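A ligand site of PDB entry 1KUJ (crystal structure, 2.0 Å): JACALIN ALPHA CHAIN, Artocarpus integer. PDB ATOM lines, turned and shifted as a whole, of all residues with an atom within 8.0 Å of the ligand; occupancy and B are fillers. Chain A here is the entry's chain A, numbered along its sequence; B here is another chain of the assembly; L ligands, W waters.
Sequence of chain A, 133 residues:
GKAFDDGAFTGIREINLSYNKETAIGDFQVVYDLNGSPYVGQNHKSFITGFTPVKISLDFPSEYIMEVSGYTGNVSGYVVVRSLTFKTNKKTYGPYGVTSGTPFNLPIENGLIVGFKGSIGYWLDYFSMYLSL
The backbone NH of Tyr 122 lies within hydrogen-bond range of an oxygen (O6) of the ligand (3.0 Å).
OD1 of Asp 125 sits at hydrogen-bond distance from O4 of the ligand (2.8 Å).
N of Trp 123 is in hydrogen-bond range of O6 of the ligand, 2.9 Å away.
An oxygen (O3) of the ligand sits at hydrogen-bond distance from the backbone NH (N) of Gly 1.
O of Trp 123 is in hydrogen-bond range of O6 of the ligand, 3.2 Å away.
Merely in contact with the ligand: Phe 47 (3.4 Å), Tyr 78 (3.3 Å) and Gly 121 (3.2 Å).
Seven residues have an atom within 4 Å of the ligand: Gly 1, Phe 47, Tyr 78, Gly 121, Tyr 122, Trp 123 and Asp 125.
The nearest printed residue that does not touch the ligand is Val 80 (4.1 Å).
The backbone carbonyl oxygen of Asp 125 lies within hydrogen-bond range of the backbone NH of Ala 17 of chain B, at 2.8 Å.
OD2 of Asp 125 lies within hydrogen-bond range of N of Gly 121.
The backbone NH of Gly 1 lies within hydrogen-bond range of the side-chain carboxylate of Asp 125, at 3.4 Å.
The backbone NH (N) of Phe 47 sits at hydrogen-bond distance from the backbone carbonyl oxygen (O) of Gly 121.
The backbone NH of Asp 125 lies within hydrogen-bond range of the backbone carbonyl oxygen of Ser 119 (2.7 Å).
The side-chain hydroxyl (OG) of Ser 46 lies within hydrogen-bond range of the backbone carbonyl oxygen (O) of Tyr 122 (2.6 Å).
Water W1 lies within hydrogen-bond range of the side-chain carboxylate (OD1) of Asp 125, the backbone carbonyl oxygen (O) of Val 79 and an oxygen (O4) of the ligand.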
ATOM      1  N   GLY A   1       8.880 -20.335  10.697  1.00  0.00           N
ATOM      2  CA  GLY A   1       7.575 -20.934  10.284  1.00  0.00           C
ATOM      3  C   GLY A   1       6.636 -20.988  11.474  1.00  0.00           C
ATOM      4  O   GLY A   1       6.824 -20.256  12.454  1.00  0.00           O
ATOM      5  N   LYS A   2       5.611 -21.843  11.390  1.00  0.00           N
ATOM      6  CA  LYS A   2       4.656 -21.986  12.473  1.00  0.00           C
ATOM      7  C   LYS A   2       5.119 -23.099  13.417  1.00  0.00           C
ATOM      8  O   LYS A   2       5.272 -24.257  13.002  1.00  0.00           O
ATOM      9  CB  LYS A   2       3.268 -22.333  11.917  1.00  0.00           C
ATOM     10  CG  LYS A   2       2.117 -22.180  12.898  1.00  0.00           C
ATOM     11  CD  LYS A   2       0.889 -22.900  12.334  1.00  0.00           C
ATOM     12  CE  LYS A   2      -0.380 -22.545  13.096  1.00  0.00           C
ATOM     13  NZ  LYS A   2      -1.526 -23.444  12.741  1.00  0.00           N
ATOM     14  N   ALA A  24      13.571 -30.253   1.035  1.00  0.00           N
ATOM     15  CA  ALA A  24      13.535 -30.828   2.379  1.00  0.00           C
ATOM     16  C   ALA A  24      12.159 -31.407   2.734  1.00  0.00           C
ATOM     17  O   ALA A  24      11.282 -31.580   1.851  1.00  0.00           O
ATOM     18  CB  ALA A  24      13.916 -29.774   3.419  1.00  0.00           C
ATOM     19  N   ILE A  25      11.978 -31.726   4.021  1.00  0.00           N
ATOM     20  CA  ILE A  25      10.730 -32.290   4.500  1.00  0.00           C
ATOM     21  C   ILE A  25       9.702 -31.138   4.543  1.00  0.00           C
ATOM     22  O   ILE A  25      10.041 -30.009   4.905  1.00  0.00           O
ATOM     23  CB  ILE A  25      10.865 -32.838   5.960  1.00  0.00           C
ATOM     24  CG1 ILE A  25      11.885 -33.984   6.049  1.00  0.00           C
ATOM     25  CG2 ILE A  25       9.508 -33.247   6.468  1.00  0.00           C
ATOM     26  CD1 ILE A  25      11.599 -35.213   5.138  1.00  0.00           C
ATOM     27  N   SER A  46       3.167 -27.386   5.367  1.00  0.00           N
ATOM     28  CA  SER A  46       4.145 -26.474   4.787  1.00  0.00           C
ATOM     29  C   SER A  46       3.348 -25.311   4.186  1.00  0.00           C
ATOM     30  O   SER A  46       2.202 -25.513   3.762  1.00  0.00           O
ATOM     31  CB  SER A  46       4.895 -27.127   3.628  1.00  0.00           C
ATOM     32  OG  SER A  46       5.516 -26.121   2.835  1.00  0.00           O
ATOM     33  N   PHE A  47       3.970 -24.135   4.140  1.00  0.00           N
ATOM     34  CA  PHE A  47       3.338 -22.944   3.541  1.00  0.00           C
ATOM     35  C   PHE A  47       3.312 -23.034   1.996  1.00  0.00           C
ATOM     36  O   PHE A  47       2.644 -22.242   1.320  1.00  0.00           O
ATOM     37  CB  PHE A  47       4.097 -21.663   3.940  1.00  0.00           C
ATOM     38  CG  PHE A  47       4.020 -21.327   5.403  1.00  0.00           C
ATOM     39  CD1 PHE A  47       3.040 -21.897   6.220  1.00  0.00           C
ATOM     40  CD2 PHE A  47       4.916 -20.427   5.955  1.00  0.00           C
ATOM     41  CE1 PHE A  47       2.956 -21.566   7.591  1.00  0.00           C
ATOM     42  CE2 PHE A  47       4.842 -20.100   7.318  1.00  0.00           C
ATOM     43  CZ  PHE A  47       3.852 -20.669   8.134  1.00  0.00           C
ATOM     44  N   ILE A  48       4.035 -24.001   1.441  1.00  0.00           N
ATOM     45  CA  ILE A  48       4.087 -24.188  -0.014  1.00  0.00           C
ATOM     46  C   ILE A  48       3.681 -25.581  -0.413  1.00  0.00           C
ATOM     47  O   ILE A  48       3.632 -26.483   0.442  1.00  0.00           O
ATOM     48  CB  ILE A  48       5.514 -23.921  -0.567  1.00  0.00           C
ATOM     49  CG1 ILE A  48       6.529 -24.852   0.124  1.00  0.00           C
ATOM     50  CG2 ILE A  48       5.890 -22.444  -0.404  1.00  0.00           C
ATOM     51  CD1 ILE A  48       7.875 -24.991  -0.632  1.00  0.00           C
ATOM     52  N   VAL A  75      18.461 -24.527   2.714  1.00  0.00           N
ATOM     53  CA  VAL A  75      17.607 -24.559   1.558  1.00  0.00           C
ATOM     54  C   VAL A  75      17.028 -23.153   1.435  1.00  0.00           C
ATOM     55  O   VAL A  75      16.297 -22.668   2.313  1.00  0.00           O
ATOM     56  CB  VAL A  75      16.505 -25.614   1.722  1.00  0.00           C
ATOM     57  CG1 VAL A  75      15.534 -25.564   0.527  1.00  0.00           C
ATOM     58  CG2 VAL A  75      17.167 -26.979   1.795  1.00  0.00           C
ATOM     59  N   SER A  76      17.424 -22.487   0.358  1.00  0.00           N
ATOM     60  CA  SER A  76      16.992 -21.118   0.094  1.00  0.00           C
ATOM     61  C   SER A  76      17.433 -20.264   1.263  1.00  0.00           C
ATOM     62  O   SER A  76      16.723 -19.367   1.670  1.00  0.00           O
ATOM     63  CB  SER A  76      15.477 -21.054  -0.066  1.00  0.00           C
ATOM     64  OG  SER A  76      15.059 -21.830  -1.186  1.00  0.00           O
ATOM     65  N   GLY A  77      18.591 -20.572   1.823  1.00  0.00           N
ATOM     66  CA  GLY A  77      19.084 -19.777   2.938  1.00  0.00           C
ATOM     67  C   GLY A  77      18.642 -20.178   4.356  1.00  0.00           C
ATOM     68  O   GLY A  77      19.098 -19.588   5.334  1.00  0.00           O
ATOM     69  N   TYR A  78      17.767 -21.183   4.463  1.00  0.00           N
ATOM     70  CA  TYR A  78      17.254 -21.637   5.761  1.00  0.00           C
ATOM     71  C   TYR A  78      17.816 -23.001   6.202  1.00  0.00           C
ATOM     72  O   TYR A  78      17.863 -23.937   5.412  1.00  0.00           O
ATOM     73  CB  TYR A  78      15.720 -21.704   5.707  1.00  0.00           C
ATOM     74  CG  TYR A  78      15.087 -20.347   5.557  1.00  0.00           C
ATOM     75  CD1 TYR A  78      14.847 -19.560   6.674  1.00  0.00           C
ATOM     76  CD2 TYR A  78      14.771 -19.819   4.296  1.00  0.00           C
ATOM     77  CE1 TYR A  78      14.321 -18.292   6.564  1.00  0.00           C
ATOM     78  CE2 TYR A  78      14.240 -18.523   4.169  1.00  0.00           C
ATOM     79  CZ  TYR A  78      14.021 -17.772   5.327  1.00  0.00           C
ATOM     80  OH  TYR A  78      13.476 -16.511   5.277  1.00  0.00           O
ATOM     81  N   VAL A  79      18.253 -23.106   7.462  1.00  0.00           N
ATOM     82  CA  VAL A  79      18.758 -24.405   7.936  1.00  0.00           C
ATOM     83  C   VAL A  79      17.504 -25.181   8.262  1.00  0.00           C
ATOM     84  O   VAL A  79      16.745 -24.810   9.170  1.00  0.00           O
ATOM     85  CB  VAL A  79      19.651 -24.324   9.219  1.00  0.00           C
ATOM     86  CG1 VAL A  79      20.059 -25.767   9.670  1.00  0.00           C
ATOM     87  CG2 VAL A  79      20.910 -23.529   8.941  1.00  0.00           C
ATOM     88  N   VAL A  80      17.304 -26.268   7.516  1.00  0.00           N
ATOM     89  CA  VAL A  80      16.126 -27.106   7.679  1.00  0.00           C
ATOM     90  C   VAL A  80      16.406 -28.613   7.749  1.00  0.00           C
ATOM     91  O   VAL A  80      17.529 -29.059   7.543  1.00  0.00           O
ATOM     92  CB  VAL A  80      15.142 -26.793   6.511  1.00  0.00           C
ATOM     93  CG1 VAL A  80      14.670 -25.339   6.616  1.00  0.00           C
ATOM     94  CG2 VAL A  80      15.884 -26.945   5.167  1.00  0.00           C
ATOM     95  N   VAL A  81      15.394 -29.401   8.084  1.00  0.00           N
ATOM     96  CA  VAL A  81      15.542 -30.855   8.118  1.00  0.00           C
ATOM     97  C   VAL A  81      15.266 -31.286   6.697  1.00  0.00           C
ATOM     98  O   VAL A  81      14.131 -31.190   6.234  1.00  0.00           O
ATOM     99  CB  VAL A  81      14.487 -31.506   9.047  1.00  0.00           C
ATOM    100  CG1 VAL A  81      14.570 -33.068   8.942  1.00  0.00           C
ATOM    101  CG2 VAL A  81      14.691 -30.991  10.474  1.00  0.00           C
ATOM    102  N   SER A 119       8.868 -26.920  14.207  1.00  0.00           N
ATOM    103  CA  SER A 119       8.384 -25.731  13.491  1.00  0.00           C
ATOM    104  C   SER A 119       8.455 -25.981  11.990  1.00  0.00           C
ATOM    105  O   SER A 119       9.449 -26.566  11.490  1.00  0.00           O
ATOM    106  CB  SER A 119       9.240 -24.511  13.862  1.00  0.00           C
ATOM    107  OG  SER A 119       8.766 -23.332  13.211  1.00  0.00           O
ATOM    108  N   ILE A 120       7.402 -25.551  11.283  1.00  0.00           N
ATOM    109  CA  ILE A 120       7.328 -25.690   9.825  1.00  0.00           C
ATOM    110  C   ILE A 120       6.937 -24.364   9.144  1.00  0.00           C
ATOM    111  O   ILE A 120       5.918 -23.731   9.497  1.00  0.00           O
ATOM    112  CB  ILE A 120       6.292 -26.782   9.398  1.00  0.00           C
ATOM    113  CG1 ILE A 120       6.681 -28.158   9.977  1.00  0.00           C
ATOM    114  CG2 ILE A 120       6.306 -26.948   7.863  1.00  0.00           C
ATOM    115  CD1 ILE A 120       5.631 -29.275   9.626  1.00  0.00           C
ATOM    116  N   GLY A 121       7.775 -23.942   8.196  1.00  0.00           N
ATOM    117  CA  GLY A 121       7.517 -22.753   7.382  1.00  0.00           C
ATOM    118  C   GLY A 121       7.303 -23.324   5.976  1.00  0.00           C
ATOM    119  O   GLY A 121       6.317 -24.016   5.751  1.00  0.00           O
ATOM    120  N   TYR A 122       8.231 -23.065   5.051  1.00  0.00           N
ATOM    121  CA  TYR A 122       8.176 -23.677   3.712  1.00  0.00           C
ATOM    122  C   TYR A 122       8.568 -25.158   3.953  1.00  0.00           C
ATOM    123  O   TYR A 122       8.115 -26.085   3.260  1.00  0.00           O
ATOM    124  CB  TYR A 122       9.229 -23.046   2.787  1.00  0.00           C
ATOM    125  CG  TYR A 122       8.792 -21.778   2.091  1.00  0.00           C
ATOM    126  CD1 TYR A 122       7.765 -21.007   2.622  1.00  0.00           C
ATOM    127  CD2 TYR A 122       9.389 -21.370   0.884  1.00  0.00           C
ATOM    128  CE1 TYR A 122       7.329 -19.854   1.970  1.00  0.00           C
ATOM    129  CE2 TYR A 122       8.954 -20.207   0.231  1.00  0.00           C
ATOM    130  CZ  TYR A 122       7.922 -19.464   0.776  1.00  0.00           C
ATOM    131  OH  TYR A 122       7.457 -18.316   0.184  1.00  0.00           O
ATOM    132  N   TRP A 123       9.426 -25.361   4.951  1.00  0.00           N
ATOM    133  CA  TRP A 123       9.901 -26.712   5.288  1.00  0.00           C
ATOM    134  C   TRP A 123       9.966 -26.944   6.790  1.00  0.00           C
ATOM    135  O   TRP A 123       9.701 -26.037   7.592  1.00  0.00           O
ATOM    136  CB  TRP A 123      11.298 -26.958   4.661  1.00  0.00           C
ATOM    137  CG  TRP A 123      11.297 -26.775   3.167  1.00  0.00           C
ATOM    138  CD1 TRP A 123      10.766 -27.627   2.213  1.00  0.00           C
ATOM    139  CD2 TRP A 123      11.771 -25.628   2.463  1.00  0.00           C
ATOM    140  NE1 TRP A 123      10.891 -27.059   0.952  1.00  0.00           N
ATOM    141  CE2 TRP A 123      11.507 -25.829   1.079  1.00  0.00           C
ATOM    142  CE3 TRP A 123      12.397 -24.431   2.864  1.00  0.00           C
ATOM    143  CZ2 TRP A 123      11.852 -24.891   0.096  1.00  0.00           C
ATOM    144  CZ3 TRP A 123      12.754 -23.486   1.871  1.00  0.00           C
ATOM    145  CH2 TRP A 123      12.481 -23.731   0.515  1.00  0.00           C
ATOM    146  N   LEU A 124      10.276 -28.180   7.177  1.00  0.00           N
ATOM    147  CA  LEU A 124      10.396 -28.464   8.603  1.00  0.00           C
ATOM    148  C   LEU A 124      11.706 -27.813   9.027  1.00  0.00           C
ATOM    149  O   LEU A 124      12.787 -28.226   8.635  1.00  0.00           O
ATOM    150  CB  LEU A 124      10.420 -29.989   8.823  1.00  0.00           C
ATOM    151  CG  LEU A 124      10.689 -30.445  10.269  1.00  0.00           C
ATOM    152  CD1 LEU A 124       9.557 -30.064  11.165  1.00  0.00           C
ATOM    153  CD2 LEU A 124      10.832 -31.963  10.285  1.00  0.00           C
ATOM    154  N   ASP A 125      11.597 -26.740   9.793  1.00  0.00           N
ATOM    155  CA  ASP A 125      12.789 -26.012  10.259  1.00  0.00           C
ATOM    156  C   ASP A 125      13.601 -26.844  11.267  1.00  0.00           C
ATOM    157  O   ASP A 125      14.831 -26.921  11.193  1.00  0.00           O
ATOM    158  CB  ASP A 125      12.348 -24.695  10.918  1.00  0.00           C
ATOM    159  CG  ASP A 125      11.637 -23.762   9.922  1.00  0.00           C
ATOM    160  OD1 ASP A 125      12.250 -23.471   8.873  1.00  0.00           O
ATOM    161  OD2 ASP A 125      10.483 -23.341  10.191  1.00  0.00           O
ATOM    162  N   TYR A 126      12.884 -27.459  12.205  1.00  0.00           N
ATOM    163  CA  TYR A 126      13.479 -28.273  13.257  1.00  0.00           C
ATOM    164  C   TYR A 126      12.402 -29.074  13.916  1.00  0.00           C
ATOM    165  O   TYR A 126      11.211 -28.831  13.694  1.00  0.00           O
ATOM    166  CB  TYR A 126      14.177 -27.378  14.292  1.00  0.00           C
ATOM    167  CG  TYR A 126      13.287 -26.337  14.948  1.00  0.00           C
ATOM    168  CD1 TYR A 126      12.434 -26.673  16.009  1.00  0.00           C
ATOM    169  CD2 TYR A 126      13.319 -25.002  14.526  1.00  0.00           C
ATOM    170  CE1 TYR A 126      11.632 -25.703  16.627  1.00  0.00           C
ATOM    171  CE2 TYR A 126      12.518 -24.020  15.152  1.00  0.00           C
ATOM    172  CZ  TYR A 126      11.684 -24.385  16.191  1.00  0.00           C
ATOM    173  OH  TYR A 126      10.922 -23.431  16.806  1.00  0.00           O
ATOM    174  N   ALA B  17      17.224 -26.022  12.395  1.00  0.00           N
ATOM    175  CA  ALA B  17      17.620 -24.686  12.814  1.00  0.00           C
ATOM    176  C   ALA B  17      17.583 -24.491  14.320  1.00  0.00           C
ATOM    177  O   ALA B  17      16.649 -24.920  14.991  1.00  0.00           O
ATOM    178  CB  ALA B  17      16.724 -23.641  12.164  1.00  0.00           C
HETATM  179  C1  LIG L   1       9.580 -19.387   5.204  1.00  0.00           C
HETATM  180  C2  LIG L   1       9.242 -18.852   6.597  1.00  0.00           C
HETATM  181  C3  LIG L   1      10.462 -19.056   7.543  1.00  0.00           C
HETATM  182  C4  LIG L   1      10.956 -20.531   7.559  1.00  0.00           C
HETATM  183  C5  LIG L   1      11.324 -20.957   6.115  1.00  0.00           C
HETATM  184  C6  LIG L   1      11.820 -22.409   5.983  1.00  0.00           C
HETATM  185  C7  LIG L   1      11.026 -18.781   3.291  1.00  0.00           C
HETATM  186  O1  LIG L   1      10.605 -18.546   4.664  1.00  0.00           O
HETATM  187  O2  LIG L   1       8.170 -19.599   7.112  1.00  0.00           O
HETATM  188  O3  LIG L   1      10.101 -18.598   8.889  1.00  0.00           O
HETATM  189  O4  LIG L   1      12.093 -20.690   8.405  1.00  0.00           O
HETATM  190  O5  LIG L   1      10.139 -20.759   5.277  1.00  0.00           O
HETATM  191  O6  LIG L   1      10.839 -23.339   6.412  1.00  0.00           O
HETATM  192  O   HOH W   1      14.629 -22.782   9.161  1.00  0.00           O
